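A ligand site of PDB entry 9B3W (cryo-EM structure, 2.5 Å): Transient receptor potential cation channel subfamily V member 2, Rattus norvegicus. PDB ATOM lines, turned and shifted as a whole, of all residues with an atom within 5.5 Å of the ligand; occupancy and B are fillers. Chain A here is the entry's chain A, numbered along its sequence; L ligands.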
ATOM      1  N   PHE A 395     -14.765  16.195  13.781  1.00  0.00           N
ATOM      2  CA  PHE A 395     -14.288  14.845  14.092  1.00  0.00           C
ATOM      3  C   PHE A 395     -13.425  14.300  12.960  1.00  0.00           C
ATOM      4  O   PHE A 395     -12.399  13.653  13.204  1.00  0.00           O
ATOM      5  CB  PHE A 395     -15.477  13.920  14.347  1.00  0.00           C
ATOM      6  CG  PHE A 395     -15.096  12.473  14.492  1.00  0.00           C
ATOM      7  CD1 PHE A 395     -14.371  12.046  15.600  1.00  0.00           C
ATOM      8  CD2 PHE A 395     -15.464  11.550  13.541  1.00  0.00           C
ATOM      9  CE1 PHE A 395     -14.022  10.715  15.736  1.00  0.00           C
ATOM     10  CE2 PHE A 395     -15.115  10.219  13.676  1.00  0.00           C
ATOM     11  CZ  PHE A 395     -14.396   9.797  14.773  1.00  0.00           C
ATOM     12  N   ASN A 396     -13.820  14.551  11.705  1.00  0.00           N
ATOM     13  CA  ASN A 396     -12.996  14.179  10.568  1.00  0.00           C
ATOM     14  C   ASN A 396     -11.659  14.922  10.582  1.00  0.00           C
ATOM     15  O   ASN A 396     -10.603  14.346  10.275  1.00  0.00           O
ATOM     16  CB  ASN A 396     -13.732  14.457   9.263  1.00  0.00           C
ATOM     17  CG  ASN A 396     -14.971  13.605   9.100  1.00  0.00           C
ATOM     18  OD1 ASN A 396     -15.236  12.707   9.908  1.00  0.00           O
ATOM     19  ND2 ASN A 396     -15.748  13.871   8.065  1.00  0.00           N
ATOM     20  N   PHE A 397     -11.694  16.209  10.960  1.00  0.00           N
ATOM     21  CA  PHE A 397     -10.455  16.978  11.094  1.00  0.00           C
ATOM     22  C   PHE A 397      -9.548  16.399  12.180  1.00  0.00           C
ATOM     23  O   PHE A 397      -8.334  16.326  12.003  1.00  0.00           O
ATOM     24  CB  PHE A 397     -10.784  18.444  11.398  1.00  0.00           C
ATOM     25  CG  PHE A 397      -9.585  19.262  11.776  1.00  0.00           C
ATOM     26  CD1 PHE A 397      -8.481  19.335  10.937  1.00  0.00           C
ATOM     27  CD2 PHE A 397      -9.555  19.953  12.968  1.00  0.00           C
ATOM     28  CE1 PHE A 397      -7.382  20.094  11.279  1.00  0.00           C
ATOM     29  CE2 PHE A 397      -8.450  20.706  13.321  1.00  0.00           C
ATOM     30  CZ  PHE A 397      -7.364  20.780  12.466  1.00  0.00           C
ATOM     31  N   CYS A 399      -9.485  13.262  13.238  1.00  0.00           N
ATOM     32  CA  CYS A 399      -8.935  12.002  12.739  1.00  0.00           C
ATOM     33  C   CYS A 399      -7.789  12.232  11.771  1.00  0.00           C
ATOM     34  O   CYS A 399      -6.771  11.534  11.818  1.00  0.00           O
ATOM     35  CB  CYS A 399     -10.040  11.176  12.073  1.00  0.00           C
ATOM     36  SG  CYS A 399     -11.257  10.502  13.218  1.00  0.00           S
ATOM     37  N   TYR A 400      -7.921  13.232  10.881  1.00  0.00           N
ATOM     38  CA  TYR A 400      -6.829  13.517   9.965  1.00  0.00           C
ATOM     39  C   TYR A 400      -5.613  14.091  10.693  1.00  0.00           C
ATOM     40  O   TYR A 400      -4.473  13.823  10.294  1.00  0.00           O
ATOM     41  CB  TYR A 400      -7.297  14.467   8.861  1.00  0.00           C
ATOM     42  CG  TYR A 400      -6.346  14.495   7.687  1.00  0.00           C
ATOM     43  CD1 TYR A 400      -6.199  13.385   6.866  1.00  0.00           C
ATOM     44  CD2 TYR A 400      -5.591  15.616   7.400  1.00  0.00           C
ATOM     45  CE1 TYR A 400      -5.333  13.391   5.800  1.00  0.00           C
ATOM     46  CE2 TYR A 400      -4.718  15.632   6.326  1.00  0.00           C
ATOM     47  CZ  TYR A 400      -4.601  14.518   5.528  1.00  0.00           C
ATOM     48  OH  TYR A 400      -3.731  14.533   4.463  1.00  0.00           O
ATOM     49  N   VAL A 402      -4.717  13.244  13.769  1.00  0.00           N
ATOM     50  CA  VAL A 402      -4.088  12.098  14.409  1.00  0.00           C
ATOM     51  C   VAL A 402      -3.273  11.303  13.385  1.00  0.00           C
ATOM     52  O   VAL A 402      -2.120  10.921  13.642  1.00  0.00           O
ATOM     53  CB  VAL A 402      -5.147  11.218  15.088  1.00  0.00           C
ATOM     54  CG1 VAL A 402      -4.578   9.858  15.467  1.00  0.00           C
ATOM     55  CG2 VAL A 402      -5.697  11.917  16.321  1.00  0.00           C
ATOM     56  N   TYR A 403      -3.853  11.082  12.205  1.00  0.00           N
ATOM     57  CA  TYR A 403      -3.174  10.343  11.145  1.00  0.00           C
ATOM     58  C   TYR A 403      -1.906  11.068  10.694  1.00  0.00           C
ATOM     59  O   TYR A 403      -0.856  10.446  10.496  1.00  0.00           O
ATOM     60  CB  TYR A 403      -4.128  10.136   9.977  1.00  0.00           C
ATOM     61  CG  TYR A 403      -3.485   9.666   8.690  1.00  0.00           C
ATOM     62  CD1 TYR A 403      -3.037   8.367   8.554  1.00  0.00           C
ATOM     63  CD2 TYR A 403      -3.348  10.535   7.619  1.00  0.00           C
ATOM     64  CE1 TYR A 403      -2.462   7.934   7.376  1.00  0.00           C
ATOM     65  CE2 TYR A 403      -2.761  10.122   6.435  1.00  0.00           C
ATOM     66  CZ  TYR A 403      -2.323   8.820   6.328  1.00  0.00           C
ATOM     67  OH  TYR A 403      -1.743   8.396   5.151  1.00  0.00           O
ATOM     68  N   GLY A 444      -4.373   3.795   7.030  1.00  0.00           N
ATOM     69  CA  GLY A 444      -4.948   5.094   6.779  1.00  0.00           C
ATOM     70  C   GLY A 444      -4.869   5.500   5.318  1.00  0.00           C
ATOM     71  O   GLY A 444      -5.800   6.117   4.785  1.00  0.00           O
ATOM     72  N   TYR A 447      -7.554   3.548   3.527  1.00  0.00           N
ATOM     73  CA  TYR A 447      -8.862   4.123   3.830  1.00  0.00           C
ATOM     74  C   TYR A 447      -9.107   5.398   3.016  1.00  0.00           C
ATOM     75  O   TYR A 447     -10.174   5.566   2.418  1.00  0.00           O
ATOM     76  CB  TYR A 447      -8.955   4.404   5.332  1.00  0.00           C
ATOM     77  CG  TYR A 447     -10.307   4.890   5.812  1.00  0.00           C
ATOM     78  CD1 TYR A 447     -11.281   3.977   6.188  1.00  0.00           C
ATOM     79  CD2 TYR A 447     -10.604   6.251   5.885  1.00  0.00           C
ATOM     80  CE1 TYR A 447     -12.512   4.409   6.627  1.00  0.00           C
ATOM     81  CE2 TYR A 447     -11.835   6.682   6.324  1.00  0.00           C
ATOM     82  CZ  TYR A 447     -12.789   5.761   6.695  1.00  0.00           C
ATOM     83  OH  TYR A 447     -14.018   6.171   7.132  1.00  0.00           O
ATOM     84  N   LEU A 448      -8.116   6.301   2.992  1.00  0.00           N
ATOM     85  CA  LEU A 448      -8.265   7.544   2.236  1.00  0.00           C
ATOM     86  C   LEU A 448      -8.358   7.285   0.742  1.00  0.00           C
ATOM     87  O   LEU A 448      -9.095   7.962   0.022  1.00  0.00           O
ATOM     88  CB  LEU A 448      -7.116   8.487   2.559  1.00  0.00           C
ATOM     89  CG  LEU A 448      -7.151   9.127   3.946  1.00  0.00           C
ATOM     90  CD1 LEU A 448      -5.818   9.760   4.295  1.00  0.00           C
ATOM     91  CD2 LEU A 448      -8.267  10.152   4.016  1.00  0.00           C
ATOM     92  N   GLN A 452     -11.542   8.395  -1.546  1.00  0.00           N
ATOM     93  CA  GLN A 452     -11.413   9.260  -2.725  1.00  0.00           C
ATOM     94  C   GLN A 452     -11.843   8.550  -4.001  1.00  0.00           C
ATOM     95  O   GLN A 452     -12.425   9.198  -4.885  1.00  0.00           O
ATOM     96  CB  GLN A 452      -9.976   9.758  -2.851  1.00  0.00           C
ATOM     97  CG  GLN A 452      -9.584  10.753  -1.770  1.00  0.00           C
ATOM     98  CD  GLN A 452     -10.606  11.865  -1.631  1.00  0.00           C
ATOM     99  OE1 GLN A 452     -11.320  11.944  -0.635  1.00  0.00           O
ATOM    100  NE2 GLN A 452     -10.670  12.738  -2.627  1.00  0.00           N
ATOM    101  N   PHE A 472      -8.624  19.863  -3.682  1.00  0.00           N
ATOM    102  CA  PHE A 472      -8.235  19.089  -2.512  1.00  0.00           C
ATOM    103  C   PHE A 472      -8.644  17.629  -2.614  1.00  0.00           C
ATOM    104  O   PHE A 472      -8.010  16.778  -2.006  1.00  0.00           O
ATOM    105  CB  PHE A 472      -8.823  19.707  -1.246  1.00  0.00           C
ATOM    106  CG  PHE A 472      -7.952  20.755  -0.621  1.00  0.00           C
ATOM    107  CD1 PHE A 472      -6.693  20.431  -0.136  1.00  0.00           C
ATOM    108  CD2 PHE A 472      -8.384  22.067  -0.521  1.00  0.00           C
ATOM    109  CE1 PHE A 472      -5.891  21.401   0.429  1.00  0.00           C
ATOM    110  CE2 PHE A 472      -7.585  23.036   0.053  1.00  0.00           C
ATOM    111  CZ  PHE A 472      -6.330  22.695   0.524  1.00  0.00           C
ATOM    112  N   GLU A 473      -9.683  17.315  -3.398  1.00  0.00           N
ATOM    113  CA  GLU A 473     -10.020  15.917  -3.660  1.00  0.00           C
ATOM    114  C   GLU A 473      -8.897  15.230  -4.431  1.00  0.00           C
ATOM    115  O   GLU A 473      -8.488  14.112  -4.077  1.00  0.00           O
ATOM    116  CB  GLU A 473     -11.330  15.842  -4.442  1.00  0.00           C
ATOM    117  CG  GLU A 473     -12.465  16.649  -3.831  1.00  0.00           C
ATOM    118  CD  GLU A 473     -13.026  16.043  -2.571  1.00  0.00           C
ATOM    119  OE1 GLU A 473     -12.842  14.819  -2.350  1.00  0.00           O
ATOM    120  OE2 GLU A 473     -13.660  16.772  -1.792  1.00  0.00           O
ATOM    121  N   PHE A 476      -5.910  14.848  -1.986  1.00  0.00           N
ATOM    122  CA  PHE A 476      -6.094  13.749  -1.036  1.00  0.00           C
ATOM    123  C   PHE A 476      -5.909  12.399  -1.710  1.00  0.00           C
ATOM    124  O   PHE A 476      -5.293  11.488  -1.146  1.00  0.00           O
ATOM    125  CB  PHE A 476      -7.477  13.843  -0.393  1.00  0.00           C
ATOM    126  CG  PHE A 476      -7.485  14.589   0.918  1.00  0.00           C
ATOM    127  CD1 PHE A 476      -7.557  15.971   0.957  1.00  0.00           C
ATOM    128  CD2 PHE A 476      -7.451  13.904   2.123  1.00  0.00           C
ATOM    129  CE1 PHE A 476      -7.579  16.650   2.153  1.00  0.00           C
ATOM    130  CE2 PHE A 476      -7.465  14.579   3.321  1.00  0.00           C
ATOM    131  CZ  PHE A 476      -7.535  15.954   3.339  1.00  0.00           C
ATOM    132  N   TYR A 514      -7.345  22.115   4.096  1.00  0.00           N
ATOM    133  CA  TYR A 514      -8.728  21.944   3.672  1.00  0.00           C
ATOM    134  C   TYR A 514      -9.693  22.340   4.778  1.00  0.00           C
ATOM    135  O   TYR A 514     -10.745  22.931   4.531  1.00  0.00           O
ATOM    136  CB  TYR A 514      -8.964  20.483   3.256  1.00  0.00           C
ATOM    137  CG  TYR A 514     -10.413  20.133   3.056  1.00  0.00           C
ATOM    138  CD1 TYR A 514     -11.079  20.460   1.882  1.00  0.00           C
ATOM    139  CD2 TYR A 514     -11.131  19.457   4.039  1.00  0.00           C
ATOM    140  CE1 TYR A 514     -12.402  20.141   1.694  1.00  0.00           C
ATOM    141  CE2 TYR A 514     -12.468  19.141   3.867  1.00  0.00           C
ATOM    142  CZ  TYR A 514     -13.090  19.484   2.688  1.00  0.00           C
ATOM    143  OH  TYR A 514     -14.417  19.157   2.497  1.00  0.00           O
ATOM    144  N   TYR A 515      -9.327  22.024   6.028  1.00  0.00           N
ATOM    145  CA  TYR A 515     -10.237  22.192   7.150  1.00  0.00           C
ATOM    146  C   TYR A 515     -10.276  23.608   7.698  1.00  0.00           C
ATOM    147  O   TYR A 515     -10.934  23.835   8.715  1.00  0.00           O
ATOM    148  CB  TYR A 515      -9.853  21.219   8.268  1.00  0.00           C
ATOM    149  CG  TYR A 515      -9.942  19.773   7.846  1.00  0.00           C
ATOM    150  CD1 TYR A 515     -11.160  19.104   7.865  1.00  0.00           C
ATOM    151  CD2 TYR A 515      -8.814  19.079   7.434  1.00  0.00           C
ATOM    152  CE1 TYR A 515     -11.243  17.782   7.479  1.00  0.00           C
ATOM    153  CE2 TYR A 515      -8.897  17.756   7.047  1.00  0.00           C
ATOM    154  CZ  TYR A 515     -10.112  17.118   7.070  1.00  0.00           C
ATOM    155  OH  TYR A 515     -10.199  15.795   6.693  1.00  0.00           O
ATOM    156  N   TYR A 675     -20.081   7.763   4.977  1.00  0.00           N
ATOM    157  CA  TYR A 675     -18.777   7.268   4.576  1.00  0.00           C
ATOM    158  C   TYR A 675     -18.962   6.177   3.528  1.00  0.00           C
ATOM    159  O   TYR A 675     -20.077   5.730   3.265  1.00  0.00           O
ATOM    160  CB  TYR A 675     -17.978   6.734   5.770  1.00  0.00           C
ATOM    161  CG  TYR A 675     -17.732   7.758   6.851  1.00  0.00           C
ATOM    162  CD1 TYR A 675     -17.012   8.911   6.588  1.00  0.00           C
ATOM    163  CD2 TYR A 675     -18.239   7.569   8.127  1.00  0.00           C
ATOM    164  CE1 TYR A 675     -16.784   9.852   7.581  1.00  0.00           C
ATOM    165  CE2 TYR A 675     -18.022   8.514   9.127  1.00  0.00           C
ATOM    166  CZ  TYR A 675     -17.296   9.647   8.843  1.00  0.00           C
ATOM    167  OH  TYR A 675     -17.073  10.570   9.823  1.00  0.00           O
ATOM    168  N   TRP A 676     -17.847   5.768   2.919  1.00  0.00           N
ATOM    169  CA  TRP A 676     -17.903   4.695   1.934  1.00  0.00           C
ATOM    170  C   TRP A 676     -18.251   3.359   2.579  1.00  0.00           C
ATOM    171  O   TRP A 676     -18.850   2.499   1.930  1.00  0.00           O
ATOM    172  CB  TRP A 676     -16.562   4.600   1.184  1.00  0.00           C
ATOM    173  CG  TRP A 676     -15.385   4.288   2.055  1.00  0.00           C
ATOM    174  CD1 TRP A 676     -14.602   5.178   2.711  1.00  0.00           C
ATOM    175  CD2 TRP A 676     -14.858   2.987   2.354  1.00  0.00           C
ATOM    176  NE1 TRP A 676     -13.620   4.522   3.413  1.00  0.00           N
ATOM    177  CE2 TRP A 676     -13.763   3.172   3.205  1.00  0.00           C
ATOM    178  CE3 TRP A 676     -15.217   1.692   1.979  1.00  0.00           C
ATOM    179  CZ2 TRP A 676     -13.008   2.107   3.693  1.00  0.00           C
ATOM    180  CZ3 TRP A 676     -14.479   0.636   2.461  1.00  0.00           C
ATOM    181  CH2 TRP A 676     -13.379   0.853   3.308  1.00  0.00           C
ATOM    182  N   TRP A 677     -17.883   3.173   3.842  1.00  0.00           N
ATOM    183  CA  TRP A 677     -18.194   1.957   4.573  1.00  0.00           C
ATOM    184  C   TRP A 677     -19.479   2.058   5.383  1.00  0.00           C
ATOM    185  O   TRP A 677     -19.914   1.043   5.958  1.00  0.00           O
ATOM    186  CB  TRP A 677     -17.028   1.612   5.510  1.00  0.00           C
ATOM    187  CG  TRP A 677     -16.712   2.698   6.482  1.00  0.00           C
ATOM    188  CD1 TRP A 677     -15.913   3.783   6.269  1.00  0.00           C
ATOM    189  CD2 TRP A 677     -17.189   2.815   7.828  1.00  0.00           C
ATOM    190  NE1 TRP A 677     -15.863   4.570   7.392  1.00  0.00           N
ATOM    191  CE2 TRP A 677     -16.640   4.001   8.367  1.00  0.00           C
ATOM    192  CE3 TRP A 677     -18.022   2.042   8.630  1.00  0.00           C
ATOM    193  CZ2 TRP A 677     -16.897   4.423   9.665  1.00  0.00           C
ATOM    194  CZ3 TRP A 677     -18.287   2.469   9.925  1.00  0.00           C
ATOM    195  CH2 TRP A 677     -17.721   3.645  10.426  1.00  0.00           C
HETATM  196  O1  LIG L   1     -13.602  14.583   5.982  1.00  0.00           O
HETATM  197  O2  LIG L   1     -13.779  12.664   4.257  1.00  0.00           O
HETATM  198  P1  LIG L   1     -12.950  13.699   4.972  1.00  0.00           P
HETATM  199  O3  LIG L   1     -11.613  12.999   5.634  1.00  0.00           O
HETATM  200  C1  LIG L   1     -11.753  11.707   6.179  1.00  0.00           C
HETATM  201  C2  LIG L   1     -10.840  11.440   7.351  1.00  0.00           C
HETATM  202  C3  LIG L   1     -11.557  11.266   8.668  1.00  0.00           C
HETATM  203  O4  LIG L   1     -12.634  10.353   8.518  1.00  0.00           O
HETATM  204  C4  LIG L   1     -13.088   9.782   9.614  1.00  0.00           C
HETATM  205  O5  LIG L   1     -13.347  10.395  10.625  1.00  0.00           O
HETATM  206  C5  LIG L   1     -13.236   8.303   9.444  1.00  0.00           C
HETATM  207  C6  LIG L   1     -13.212   7.504  10.730  1.00  0.00           C
HETATM  208  C7  LIG L   1     -12.741   6.083  10.495  1.00  0.00           C
HETATM  209  C8  LIG L   1     -13.041   5.141  11.656  1.00  0.00           C
HETATM  210  C9  LIG L   1     -12.598   3.711  11.422  1.00  0.00           C
HETATM  211  C10 LIG L   1     -13.448   2.973  10.381  1.00  0.00           C
HETATM  212  C11 LIG L   1     -13.253   1.464  10.420  1.00  0.00           C
HETATM  213  C12 LIG L   1     -14.106   0.709   9.409  1.00  0.00           C
HETATM  214  C13 LIG L   1     -13.532   0.732   8.001  1.00  0.00           C
HETATM  215  O6  LIG L   1     -10.027  10.273   7.162  1.00  0.00           O
HETATM  216  C14 LIG L   1      -8.817  10.224   7.701  1.00  0.00           C
HETATM  217  O7  LIG L   1      -8.280  11.150   8.232  1.00  0.00           O
HETATM  218  C15 LIG L   1      -8.194   8.861   7.561  1.00  0.00           C
HETATM  219  C16 LIG L   1      -8.572   7.897   8.674  1.00  0.00           C
HETATM  220  C17 LIG L   1      -7.354   7.228   9.281  1.00  0.00           C
HETATM  221  C18 LIG L   1      -6.979   7.784  10.650  1.00  0.00           C
HETATM  222  C19 LIG L   1      -7.968   7.403  11.736  1.00  0.00           C
HETATM  223  C20 LIG L   1      -7.577   7.926  13.118  1.00  0.00           C
HETATM  224  C21 LIG L   1      -8.636   7.670  14.184  1.00  0.00           C
HETATM  225  C22 LIG L   1      -8.365   8.398  15.486  1.00  0.00           C
HETATM  226  C23 LIG L   1      -9.469   8.214  16.513  1.00  0.00           C
HETATM  227  O8  LIG L   1     -12.093  14.620   3.919  1.00  0.00           O
HETATM  228  C24 LIG L   1     -11.686  14.013   2.703  1.00  0.00           C
HETATM  229  C25 LIG L   1     -11.230  15.067   1.728  1.00  0.00           C
HETATM  230  N1  LIG L   1     -12.241  16.073   1.492  1.00  0.00           N
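The side-chain sulfur of Cys 399 is in hydrogen-bond range of an oxygen (O5) of the ligand, at 3.3 Å.
OE2 of Glu 473 is in salt-bridge range of N1 of the ligand, 3.6 Å away.
An oxygen (O7) of the ligand sits close to the backbone NH (N) of Tyr 400.
The side-chain amide oxygen of Asn 396 sits close to an oxygen (O5) of the ligand, 3.1 Å away.
OH of Tyr 515 is in hydrogen-bond range of O3 of the ligand.
NE1 of Trp 677 lies within hydrogen-bond range of OH of Tyr 447 (2.5 Å).
SG of Cys 399 lies within hydrogen-bond range of O of Phe 395 (3.4 Å).
O of Glu 473 is in hydrogen-bond range of NE2 of Gln 452.
OD1 of Asn 396 is in hydrogen-bond range of OH of Tyr 675 (2.8 Å).
Merely in contact with the ligand: Tyr 447 (3.2 Å), Phe 395 (3.5 Å), Leu 448 (3.6 Å), Tyr 514 (3.7 Å), Tyr 403 (3.8 Å), Trp 677 (3.8 Å), Tyr 675 (3.8 Å), Phe 476 (3.9 Å) and Gln 452 (3.9 Å).
Within 4 Å of the ligand: Phe 395, Asn 396, Cys 399, Tyr 400, Tyr 403, Tyr 447, Leu 448, Gln 452, Glu 473, Phe 476, Tyr 514, Tyr 515, Tyr 675 and Trp 677.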
